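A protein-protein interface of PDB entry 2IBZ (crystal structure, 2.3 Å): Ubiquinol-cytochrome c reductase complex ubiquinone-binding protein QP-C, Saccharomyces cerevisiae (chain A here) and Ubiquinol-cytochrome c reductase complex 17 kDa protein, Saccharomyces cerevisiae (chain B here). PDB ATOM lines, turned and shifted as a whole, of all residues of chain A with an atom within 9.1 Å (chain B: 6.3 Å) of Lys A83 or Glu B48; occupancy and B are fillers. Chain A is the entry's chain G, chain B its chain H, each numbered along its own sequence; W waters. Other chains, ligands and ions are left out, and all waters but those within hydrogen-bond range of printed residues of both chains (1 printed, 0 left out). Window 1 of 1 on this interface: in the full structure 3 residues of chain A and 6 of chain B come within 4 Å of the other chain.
A ring nitrogen (NE2) of His B46 sits at hydrogen-bond distance from the guanidinium group of Arg A86, 3.0 Å away. SG of Cys B28 is in hydrogen-bond range of NZ of Lys A83 (3.3 Å). NZ of Lys A83 lies within salt-bridge range of OE1 of Glu B53, 2.7 Å away. The side-chain amino group of Lys A83 is in hydrogen-bond range of the backbone carbonyl oxygen of Asp B49. OE2 of Glu B52 is in hydrogen-bond range of N of Lys A83. The side-chain carboxylate of Glu B48 is in salt-bridge range of the side-chain amino group of Lys A83, at 3.1 Å.
CA of Ser A82 touches OE2 of Glu B52, 3.6 Å away.
NH1 of Arg B31 lies within salt-bridge range of OE2 of Glu B48 (3.3 Å). N of Val B51 is in hydrogen-bond range of OD2 of Asp B49. The side-chain sulfur (SG) of Cys B28 forms a disulfide with the side-chain sulfur (SG) of Cys B50, at 2.0 Å. OG of Ser A82 is in hydrogen-bond range of O of Phe A79.
Printed residues of chain B that touch a printed residue of chain A: Cys B28, His B46, Glu B48, Asp B49, Glu B52 and Glu B53. Hydrophobic or aromatic side chains of chain B within 4 Å of the printed part of chain A: His B46. Among the printed residues, 7 pairs touch across the chains. Among the printed residues, Asp or Glu carboxylates within 4 Å of a Lys or Arg side-chain nitrogen of the other chain: Lys A83 with Glu B48 (3.1 Å) and Lys A83 with Glu B53 (2.7 Å).
Of the printed residues of chain B, Ser A82 touches Glu B52 (3.6 Å). Of chain B, only Cys B28, Glu B48, Asp B49, Glu B52 and Glu B53 come within 4 Å of Lys A83. Glu A88 touches none of the printed residues of chain B. Printed residues of chain A within 4 Å of Cys B28: Lys A83. Of chain A, only Lys A83 comes within 4 Å of Glu B48. Val B51 touches none of the printed residues of chain A. Of the printed residues of chain A, Glu B52 touches Ser A82 and Lys A83. Of the printed residues of chain A, Glu B53 touches Lys A83. The nearest residue of chain B that does not touch Lys A83 is Cys B50 (4.2 Å). The nearest residue of chain A that does not touch Glu B48 is Arg A86 (7.3 Å).
Water W1 lies within hydrogen-bond range of the backbone NH (N) of Ala A84 (2.7 Å), the side-chain carboxylate (OE1) of Glu B52 (2.8 Å) and the backbone NH (N) of Lys A83 (3.3 Å).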
ATOM      1  N   ASN A  77     -32.801 -17.506  -2.266  1.00  0.00           N
ATOM      2  CA  ASN A  77     -31.598 -17.759  -3.054  1.00  0.00           C
ATOM      3  C   ASN A  77     -30.516 -16.743  -2.672  1.00  0.00           C
ATOM      4  O   ASN A  77     -29.332 -17.076  -2.604  1.00  0.00           O
ATOM      5  CB  ASN A  77     -31.925 -17.669  -4.562  1.00  0.00           C
ATOM      6  CG  ASN A  77     -30.712 -17.933  -5.455  1.00  0.00           C
ATOM      7  OD1 ASN A  77     -30.068 -17.009  -5.939  1.00  0.00           O
ATOM      8  ND2 ASN A  77     -30.405 -19.192  -5.675  1.00  0.00           N
ATOM      9  N   GLU A  78     -30.944 -15.503  -2.443  1.00  0.00           N
ATOM     10  CA  GLU A  78     -30.060 -14.414  -2.064  1.00  0.00           C
ATOM     11  C   GLU A  78     -29.419 -14.762  -0.716  1.00  0.00           C
ATOM     12  O   GLU A  78     -28.203 -14.644  -0.539  1.00  0.00           O
ATOM     13  CB  GLU A  78     -30.863 -13.119  -1.972  1.00  0.00           C
ATOM     14  CG  GLU A  78     -30.050 -11.852  -2.179  1.00  0.00           C
ATOM     15  CD  GLU A  78     -30.929 -10.603  -2.264  1.00  0.00           C
ATOM     16  OE1 GLU A  78     -31.592 -10.410  -3.315  1.00  0.00           O
ATOM     17  OE2 GLU A  78     -30.962  -9.817  -1.285  1.00  0.00           O
ATOM     18  N   PHE A  79     -30.235 -15.241   0.217  1.00  0.00           N
ATOM     19  CA  PHE A  79     -29.733 -15.637   1.525  1.00  0.00           C
ATOM     20  C   PHE A  79     -28.711 -16.770   1.383  1.00  0.00           C
ATOM     21  O   PHE A  79     -27.613 -16.689   1.917  1.00  0.00           O
ATOM     22  CB  PHE A  79     -30.889 -16.073   2.427  1.00  0.00           C
ATOM     23  CG  PHE A  79     -30.457 -16.837   3.653  1.00  0.00           C
ATOM     24  CD1 PHE A  79     -29.883 -16.178   4.737  1.00  0.00           C
ATOM     25  CD2 PHE A  79     -30.642 -18.222   3.728  1.00  0.00           C
ATOM     26  CE1 PHE A  79     -29.500 -16.888   5.887  1.00  0.00           C
ATOM     27  CE2 PHE A  79     -30.262 -18.941   4.871  1.00  0.00           C
ATOM     28  CZ  PHE A  79     -29.690 -18.271   5.954  1.00  0.00           C
ATOM     29  N   LEU A  80     -29.057 -17.801   0.621  1.00  0.00           N
ATOM     30  CA  LEU A  80     -28.161 -18.935   0.430  1.00  0.00           C
ATOM     31  C   LEU A  80     -26.762 -18.573  -0.082  1.00  0.00           C
ATOM     32  O   LEU A  80     -25.787 -19.226   0.267  1.00  0.00           O
ATOM     33  CB  LEU A  80     -28.793 -19.953  -0.513  1.00  0.00           C
ATOM     34  CG  LEU A  80     -29.974 -20.775  -0.004  1.00  0.00           C
ATOM     35  CD1 LEU A  80     -30.486 -21.685  -1.124  1.00  0.00           C
ATOM     36  CD2 LEU A  80     -29.519 -21.621   1.172  1.00  0.00           C
ATOM     37  N   TYR A  81     -26.668 -17.526  -0.897  1.00  0.00           N
ATOM     38  CA  TYR A  81     -25.384 -17.131  -1.462  1.00  0.00           C
ATOM     39  C   TYR A  81     -24.654 -15.988  -0.752  1.00  0.00           C
ATOM     40  O   TYR A  81     -23.641 -15.481  -1.238  1.00  0.00           O
ATOM     41  CB  TYR A  81     -25.517 -16.918  -2.981  1.00  0.00           C
ATOM     42  CG  TYR A  81     -25.688 -18.236  -3.713  1.00  0.00           C
ATOM     43  CD1 TYR A  81     -26.953 -18.801  -3.885  1.00  0.00           C
ATOM     44  CD2 TYR A  81     -24.576 -18.969  -4.142  1.00  0.00           C
ATOM     45  CE1 TYR A  81     -27.111 -20.069  -4.456  1.00  0.00           C
ATOM     46  CE2 TYR A  81     -24.720 -20.228  -4.715  1.00  0.00           C
ATOM     47  CZ  TYR A  81     -25.992 -20.771  -4.867  1.00  0.00           C
ATOM     48  OH  TYR A  81     -26.145 -22.012  -5.429  1.00  0.00           O
ATOM     49  N   SER A  82     -25.169 -15.607   0.413  1.00  0.00           N
ATOM     50  CA  SER A  82     -24.548 -14.579   1.242  1.00  0.00           C
ATOM     51  C   SER A  82     -23.718 -15.331   2.290  1.00  0.00           C
ATOM     52  O   SER A  82     -23.788 -16.562   2.374  1.00  0.00           O
ATOM     53  CB  SER A  82     -25.611 -13.733   1.944  1.00  0.00           C
ATOM     54  OG  SER A  82     -26.354 -14.521   2.858  1.00  0.00           O
ATOM     55  N   LYS A  83     -22.925 -14.599   3.074  1.00  0.00           N
ATOM     56  CA  LYS A  83     -22.093 -15.214   4.115  1.00  0.00           C
ATOM     57  C   LYS A  83     -22.947 -15.965   5.121  1.00  0.00           C
ATOM     58  O   LYS A  83     -22.708 -17.145   5.398  1.00  0.00           O
ATOM     59  CB  LYS A  83     -21.290 -14.156   4.869  1.00  0.00           C
ATOM     60  CG  LYS A  83     -19.938 -13.837   4.276  1.00  0.00           C
ATOM     61  CD  LYS A  83     -19.148 -12.936   5.213  1.00  0.00           C
ATOM     62  CE  LYS A  83     -17.796 -12.634   4.628  1.00  0.00           C
ATOM     63  NZ  LYS A  83     -17.095 -11.570   5.383  1.00  0.00           N
ATOM     64  N   ALA A  84     -23.951 -15.269   5.648  1.00  0.00           N
ATOM     65  CA  ALA A  84     -24.861 -15.817   6.645  1.00  0.00           C
ATOM     66  C   ALA A  84     -25.479 -17.164   6.297  1.00  0.00           C
ATOM     67  O   ALA A  84     -25.793 -17.954   7.192  1.00  0.00           O
ATOM     68  CB  ALA A  84     -25.967 -14.806   6.958  1.00  0.00           C
ATOM     69  N   GLY A  85     -25.627 -17.441   5.003  1.00  0.00           N
ATOM     70  CA  GLY A  85     -26.249 -18.687   4.594  1.00  0.00           C
ATOM     71  C   GLY A  85     -25.397 -19.781   3.989  1.00  0.00           C
ATOM     72  O   GLY A  85     -25.947 -20.796   3.560  1.00  0.00           O
ATOM     73  N   ARG A  86     -24.077 -19.613   3.973  1.00  0.00           N
ATOM     74  CA  ARG A  86     -23.199 -20.624   3.386  1.00  0.00           C
ATOM     75  C   ARG A  86     -23.284 -21.966   4.098  1.00  0.00           C
ATOM     76  O   ARG A  86     -22.963 -23.006   3.524  1.00  0.00           O
ATOM     77  CB  ARG A  86     -21.742 -20.143   3.324  1.00  0.00           C
ATOM     78  CG  ARG A  86     -21.126 -19.779   4.662  1.00  0.00           C
ATOM     79  CD  ARG A  86     -19.608 -19.663   4.563  1.00  0.00           C
ATOM     80  NE  ARG A  86     -19.005 -20.886   4.029  1.00  0.00           N
ATOM     81  CZ  ARG A  86     -19.075 -22.086   4.607  1.00  0.00           C
ATOM     82  NH1 ARG A  86     -18.496 -23.132   4.029  1.00  0.00           N
ATOM     83  NH2 ARG A  86     -19.706 -22.245   5.768  1.00  0.00           N
ATOM     84  N   GLU A  87     -23.734 -21.934   5.346  1.00  0.00           N
ATOM     85  CA  GLU A  87     -23.877 -23.144   6.146  1.00  0.00           C
ATOM     86  C   GLU A  87     -25.087 -23.912   5.615  1.00  0.00           C
ATOM     87  O   GLU A  87     -24.992 -25.101   5.309  1.00  0.00           O
ATOM     88  CB  GLU A  87     -24.057 -22.773   7.621  1.00  0.00           C
ATOM     89  CG  GLU A  87     -23.674 -23.878   8.593  1.00  0.00           C
ATOM     90  CD  GLU A  87     -23.628 -23.394  10.033  1.00  0.00           C
ATOM     91  OE1 GLU A  87     -24.708 -23.263  10.655  1.00  0.00           O
ATOM     92  OE2 GLU A  87     -22.508 -23.145  10.541  1.00  0.00           O
ATOM     93  N   GLU A  88     -26.208 -23.204   5.466  1.00  0.00           N
ATOM     94  CA  GLU A  88     -27.440 -23.778   4.935  1.00  0.00           C
ATOM     95  C   GLU A  88     -27.254 -24.201   3.475  1.00  0.00           C
ATOM     96  O   GLU A  88     -27.831 -25.191   3.032  1.00  0.00           O
ATOM     97  CB  GLU A  88     -28.586 -22.771   5.037  1.00  0.00           C
ATOM     98  CG  GLU A  88     -29.854 -23.219   4.328  1.00  0.00           C
ATOM     99  CD  GLU A  88     -31.057 -23.285   5.240  1.00  0.00           C
ATOM    100  OE1 GLU A  88     -31.975 -22.452   5.072  1.00  0.00           O
ATOM    101  OE2 GLU A  88     -31.088 -24.177   6.117  1.00  0.00           O
ATOM    102  N   LEU A  89     -26.435 -23.449   2.742  1.00  0.00           N
ATOM    103  CA  LEU A  89     -26.149 -23.738   1.338  1.00  0.00           C
ATOM    104  C   LEU A  89     -25.557 -25.135   1.189  1.00  0.00           C
ATOM    105  O   LEU A  89     -26.039 -25.922   0.388  1.00  0.00           O
ATOM    106  CB  LEU A  89     -25.201 -22.676   0.751  1.00  0.00           C
ATOM    107  CG  LEU A  89     -24.830 -22.616  -0.743  1.00  0.00           C
ATOM    108  CD1 LEU A  89     -23.727 -23.598  -1.097  1.00  0.00           C
ATOM    109  CD2 LEU A  89     -26.053 -22.846  -1.598  1.00  0.00           C
ATOM    110  N   CYS B  28     -14.127  -6.762   9.567  1.00  0.00           N
ATOM    111  CA  CYS B  28     -13.982  -7.992   8.799  1.00  0.00           C
ATOM    112  C   CYS B  28     -12.517  -8.196   8.434  1.00  0.00           C
ATOM    113  O   CYS B  28     -11.991  -9.297   8.568  1.00  0.00           O
ATOM    114  CB  CYS B  28     -14.830  -7.955   7.519  1.00  0.00           C
ATOM    115  SG  CYS B  28     -14.773  -9.500   6.538  1.00  0.00           S
ATOM    116  N   ARG B  31     -10.439  -9.412  11.433  1.00  0.00           N
ATOM    117  CA  ARG B  31     -10.712 -10.826  11.661  1.00  0.00           C
ATOM    118  C   ARG B  31      -9.989 -11.736  10.665  1.00  0.00           C
ATOM    119  O   ARG B  31      -9.546 -12.826  11.021  1.00  0.00           O
ATOM    120  CB  ARG B  31     -12.228 -11.057  11.615  1.00  0.00           C
ATOM    121  CG  ARG B  31     -12.675 -12.483  11.895  1.00  0.00           C
ATOM    122  CD  ARG B  31     -14.188 -12.573  12.115  1.00  0.00           C
ATOM    123  NE  ARG B  31     -14.972 -12.193  10.939  1.00  0.00           N
ATOM    124  CZ  ARG B  31     -15.717 -11.091  10.853  1.00  0.00           C
ATOM    125  NH1 ARG B  31     -16.397 -10.833   9.742  1.00  0.00           N
ATOM    126  NH2 ARG B  31     -15.777 -10.242  11.872  1.00  0.00           N
ATOM    127  N   VAL B  32      -9.813 -11.256   9.438  1.00  0.00           N
ATOM    128  CA  VAL B  32      -9.152 -12.032   8.393  1.00  0.00           C
ATOM    129  C   VAL B  32      -7.644 -12.198   8.566  1.00  0.00           C
ATOM    130  O   VAL B  32      -7.141 -13.320   8.487  1.00  0.00           O
ATOM    131  CB  VAL B  32      -9.460 -11.462   6.987  1.00  0.00           C
ATOM    132  CG1 VAL B  32      -8.703 -12.234   5.913  1.00  0.00           C
ATOM    133  CG2 VAL B  32     -10.944 -11.542   6.715  1.00  0.00           C
ATOM    134  N   GLN B  35      -6.580 -14.673  11.105  1.00  0.00           N
ATOM    135  CA  GLN B  35      -6.736 -16.069  10.704  1.00  0.00           C
ATOM    136  C   GLN B  35      -5.591 -16.535   9.802  1.00  0.00           C
ATOM    137  O   GLN B  35      -5.291 -17.728   9.740  1.00  0.00           O
ATOM    138  CB  GLN B  35      -8.066 -16.271   9.972  1.00  0.00           C
ATOM    139  CG  GLN B  35      -9.309 -15.989  10.803  1.00  0.00           C
ATOM    140  CD  GLN B  35     -10.599 -16.210  10.025  1.00  0.00           C
ATOM    141  OE1 GLN B  35     -10.583 -16.691   8.889  1.00  0.00           O
ATOM    142  NE2 GLN B  35     -11.725 -15.859  10.636  1.00  0.00           N
ATOM    143  N   TYR B  41      -3.303 -22.246   7.612  1.00  0.00           N
ATOM    144  CA  TYR B  41      -4.140 -21.374   6.796  1.00  0.00           C
ATOM    145  C   TYR B  41      -4.174 -21.830   5.342  1.00  0.00           C
ATOM    146  O   TYR B  41      -5.189 -21.677   4.665  1.00  0.00           O
ATOM    147  CB  TYR B  41      -3.665 -19.922   6.875  1.00  0.00           C
ATOM    148  CG  TYR B  41      -4.507 -18.967   6.056  1.00  0.00           C
ATOM    149  CD1 TYR B  41      -3.999 -18.375   4.900  1.00  0.00           C
ATOM    150  CD2 TYR B  41      -5.821 -18.673   6.423  1.00  0.00           C
ATOM    151  CE1 TYR B  41      -4.778 -17.517   4.127  1.00  0.00           C
ATOM    152  CE2 TYR B  41      -6.609 -17.815   5.657  1.00  0.00           C
ATOM    153  CZ  TYR B  41      -6.081 -17.241   4.510  1.00  0.00           C
ATOM    154  OH  TYR B  41      -6.851 -16.393   3.747  1.00  0.00           O
ATOM    155  N   HIS B  46     -11.870 -23.101   3.889  1.00  0.00           N
ATOM    156  CA  HIS B  46     -12.945 -22.384   4.566  1.00  0.00           C
ATOM    157  C   HIS B  46     -12.479 -20.954   4.855  1.00  0.00           C
ATOM    158  O   HIS B  46     -12.922 -20.326   5.821  1.00  0.00           O
ATOM    159  CB  HIS B  46     -13.279 -23.104   5.880  1.00  0.00           C
ATOM    160  CG  HIS B  46     -14.740 -23.145   6.199  1.00  0.00           C
ATOM    161  ND1 HIS B  46     -15.362 -22.188   6.974  1.00  0.00           N
ATOM    162  CD2 HIS B  46     -15.699 -24.045   5.874  1.00  0.00           C
ATOM    163  CE1 HIS B  46     -16.638 -22.499   7.114  1.00  0.00           C
ATOM    164  NE2 HIS B  46     -16.869 -23.622   6.458  1.00  0.00           N
ATOM    165  N   LYS B  47     -11.587 -20.450   4.005  1.00  0.00           N
ATOM    166  CA  LYS B  47     -11.030 -19.106   4.143  1.00  0.00           C
ATOM    167  C   LYS B  47     -12.086 -18.032   3.901  1.00  0.00           C
ATOM    168  O   LYS B  47     -12.787 -18.046   2.889  1.00  0.00           O
ATOM    169  CB  LYS B  47      -9.865 -18.903   3.169  1.00  0.00           C
ATOM    170  CG  LYS B  47      -8.897 -20.077   3.085  1.00  0.00           C
ATOM    171  CD  LYS B  47      -7.765 -19.794   2.107  1.00  0.00           C
ATOM    172  CE  LYS B  47      -7.211 -21.082   1.503  1.00  0.00           C
ATOM    173  NZ  LYS B  47      -6.742 -22.054   2.527  1.00  0.00           N
ATOM    174  N   GLU B  48     -12.195 -17.107   4.844  1.00  0.00           N
ATOM    175  CA  GLU B  48     -13.156 -16.023   4.746  1.00  0.00           C
ATOM    176  C   GLU B  48     -12.537 -14.798   4.080  1.00  0.00           C
ATOM    177  O   GLU B  48     -11.350 -14.516   4.261  1.00  0.00           O
ATOM    178  CB  GLU B  48     -13.665 -15.648   6.140  1.00  0.00           C
ATOM    179  CG  GLU B  48     -14.663 -14.491   6.157  1.00  0.00           C
ATOM    180  CD  GLU B  48     -15.105 -14.097   7.559  1.00  0.00           C
ATOM    181  OE1 GLU B  48     -14.470 -14.537   8.541  1.00  0.00           O
ATOM    182  OE2 GLU B  48     -16.090 -13.337   7.681  1.00  0.00           O
ATOM    183  N   ASP B  49     -13.335 -14.111   3.267  1.00  0.00           N
ATOM    184  CA  ASP B  49     -12.894 -12.892   2.602  1.00  0.00           C
ATOM    185  C   ASP B  49     -13.886 -11.801   2.966  1.00  0.00           C
ATOM    186  O   ASP B  49     -14.915 -12.079   3.570  1.00  0.00           O
ATOM    187  CB  ASP B  49     -12.773 -13.068   1.081  1.00  0.00           C
ATOM    188  CG  ASP B  49     -14.082 -13.448   0.416  1.00  0.00           C
ATOM    189  OD1 ASP B  49     -14.135 -14.560  -0.153  1.00  0.00           O
ATOM    190  OD2 ASP B  49     -15.041 -12.637   0.433  1.00  0.00           O
ATOM    191  N   CYS B  50     -13.590 -10.565   2.593  1.00  0.00           N
ATOM    192  CA  CYS B  50     -14.467  -9.459   2.942  1.00  0.00           C
ATOM    193  C   CYS B  50     -15.114  -8.740   1.749  1.00  0.00           C
ATOM    194  O   CYS B  50     -15.474  -7.553   1.837  1.00  0.00           O
ATOM    195  CB  CYS B  50     -13.710  -8.494   3.863  1.00  0.00           C
ATOM    196  SG  CYS B  50     -13.104  -9.306   5.389  1.00  0.00           S
ATOM    197  N   VAL B  51     -15.320  -9.495   0.665  1.00  0.00           N
ATOM    198  CA  VAL B  51     -15.933  -8.972  -0.557  1.00  0.00           C
ATOM    199  C   VAL B  51     -17.330  -8.429  -0.273  1.00  0.00           C
ATOM    200  O   VAL B  51     -17.660  -7.309  -0.646  1.00  0.00           O
ATOM    201  CB  VAL B  51     -16.024 -10.059  -1.653  1.00  0.00           C
ATOM    202  CG1 VAL B  51     -16.697  -9.501  -2.896  1.00  0.00           C
ATOM    203  CG2 VAL B  51     -14.651 -10.561  -2.013  1.00  0.00           C
ATOM    204  N   GLU B  52     -18.119  -9.218   0.441  1.00  0.00           N
ATOM    205  CA  GLU B  52     -19.478  -8.857   0.797  1.00  0.00           C
ATOM    206  C   GLU B  52     -19.512  -7.510   1.509  1.00  0.00           C
ATOM    207  O   GLU B  52     -20.213  -6.596   1.076  1.00  0.00           O
ATOM    208  CB  GLU B  52     -20.090  -9.962   1.659  1.00  0.00           C
ATOM    209  CG  GLU B  52     -21.547  -9.762   2.013  1.00  0.00           C
ATOM    210  CD  GLU B  52     -22.225 -11.053   2.456  1.00  0.00           C
ATOM    211  OE1 GLU B  52     -23.007 -11.007   3.426  1.00  0.00           O
ATOM    212  OE2 GLU B  52     -21.984 -12.116   1.834  1.00  0.00           O
ATOM    213  N   GLU B  53     -18.725  -7.381   2.577  1.00  0.00           N
ATOM    214  CA  GLU B  53     -18.646  -6.137   3.347  1.00  0.00           C
ATOM    215  C   GLU B  53     -18.137  -5.009   2.454  1.00  0.00           C
ATOM    216  O   GLU B  53     -18.604  -3.873   2.546  1.00  0.00           O
ATOM    217  CB  GLU B  53     -17.725  -6.297   4.563  1.00  0.00           C
ATOM    218  CG  GLU B  53     -18.272  -7.191   5.675  1.00  0.00           C
ATOM    219  CD  GLU B  53     -18.173  -8.674   5.359  1.00  0.00           C
ATOM    220  OE1 GLU B  53     -17.431  -9.050   4.422  1.00  0.00           O
ATOM    221  OE2 GLU B  53     -18.831  -9.469   6.063  1.00  0.00           O
HETATM  222  O   HOH W   1     -24.424 -12.618   5.188  1.00  0.00           O
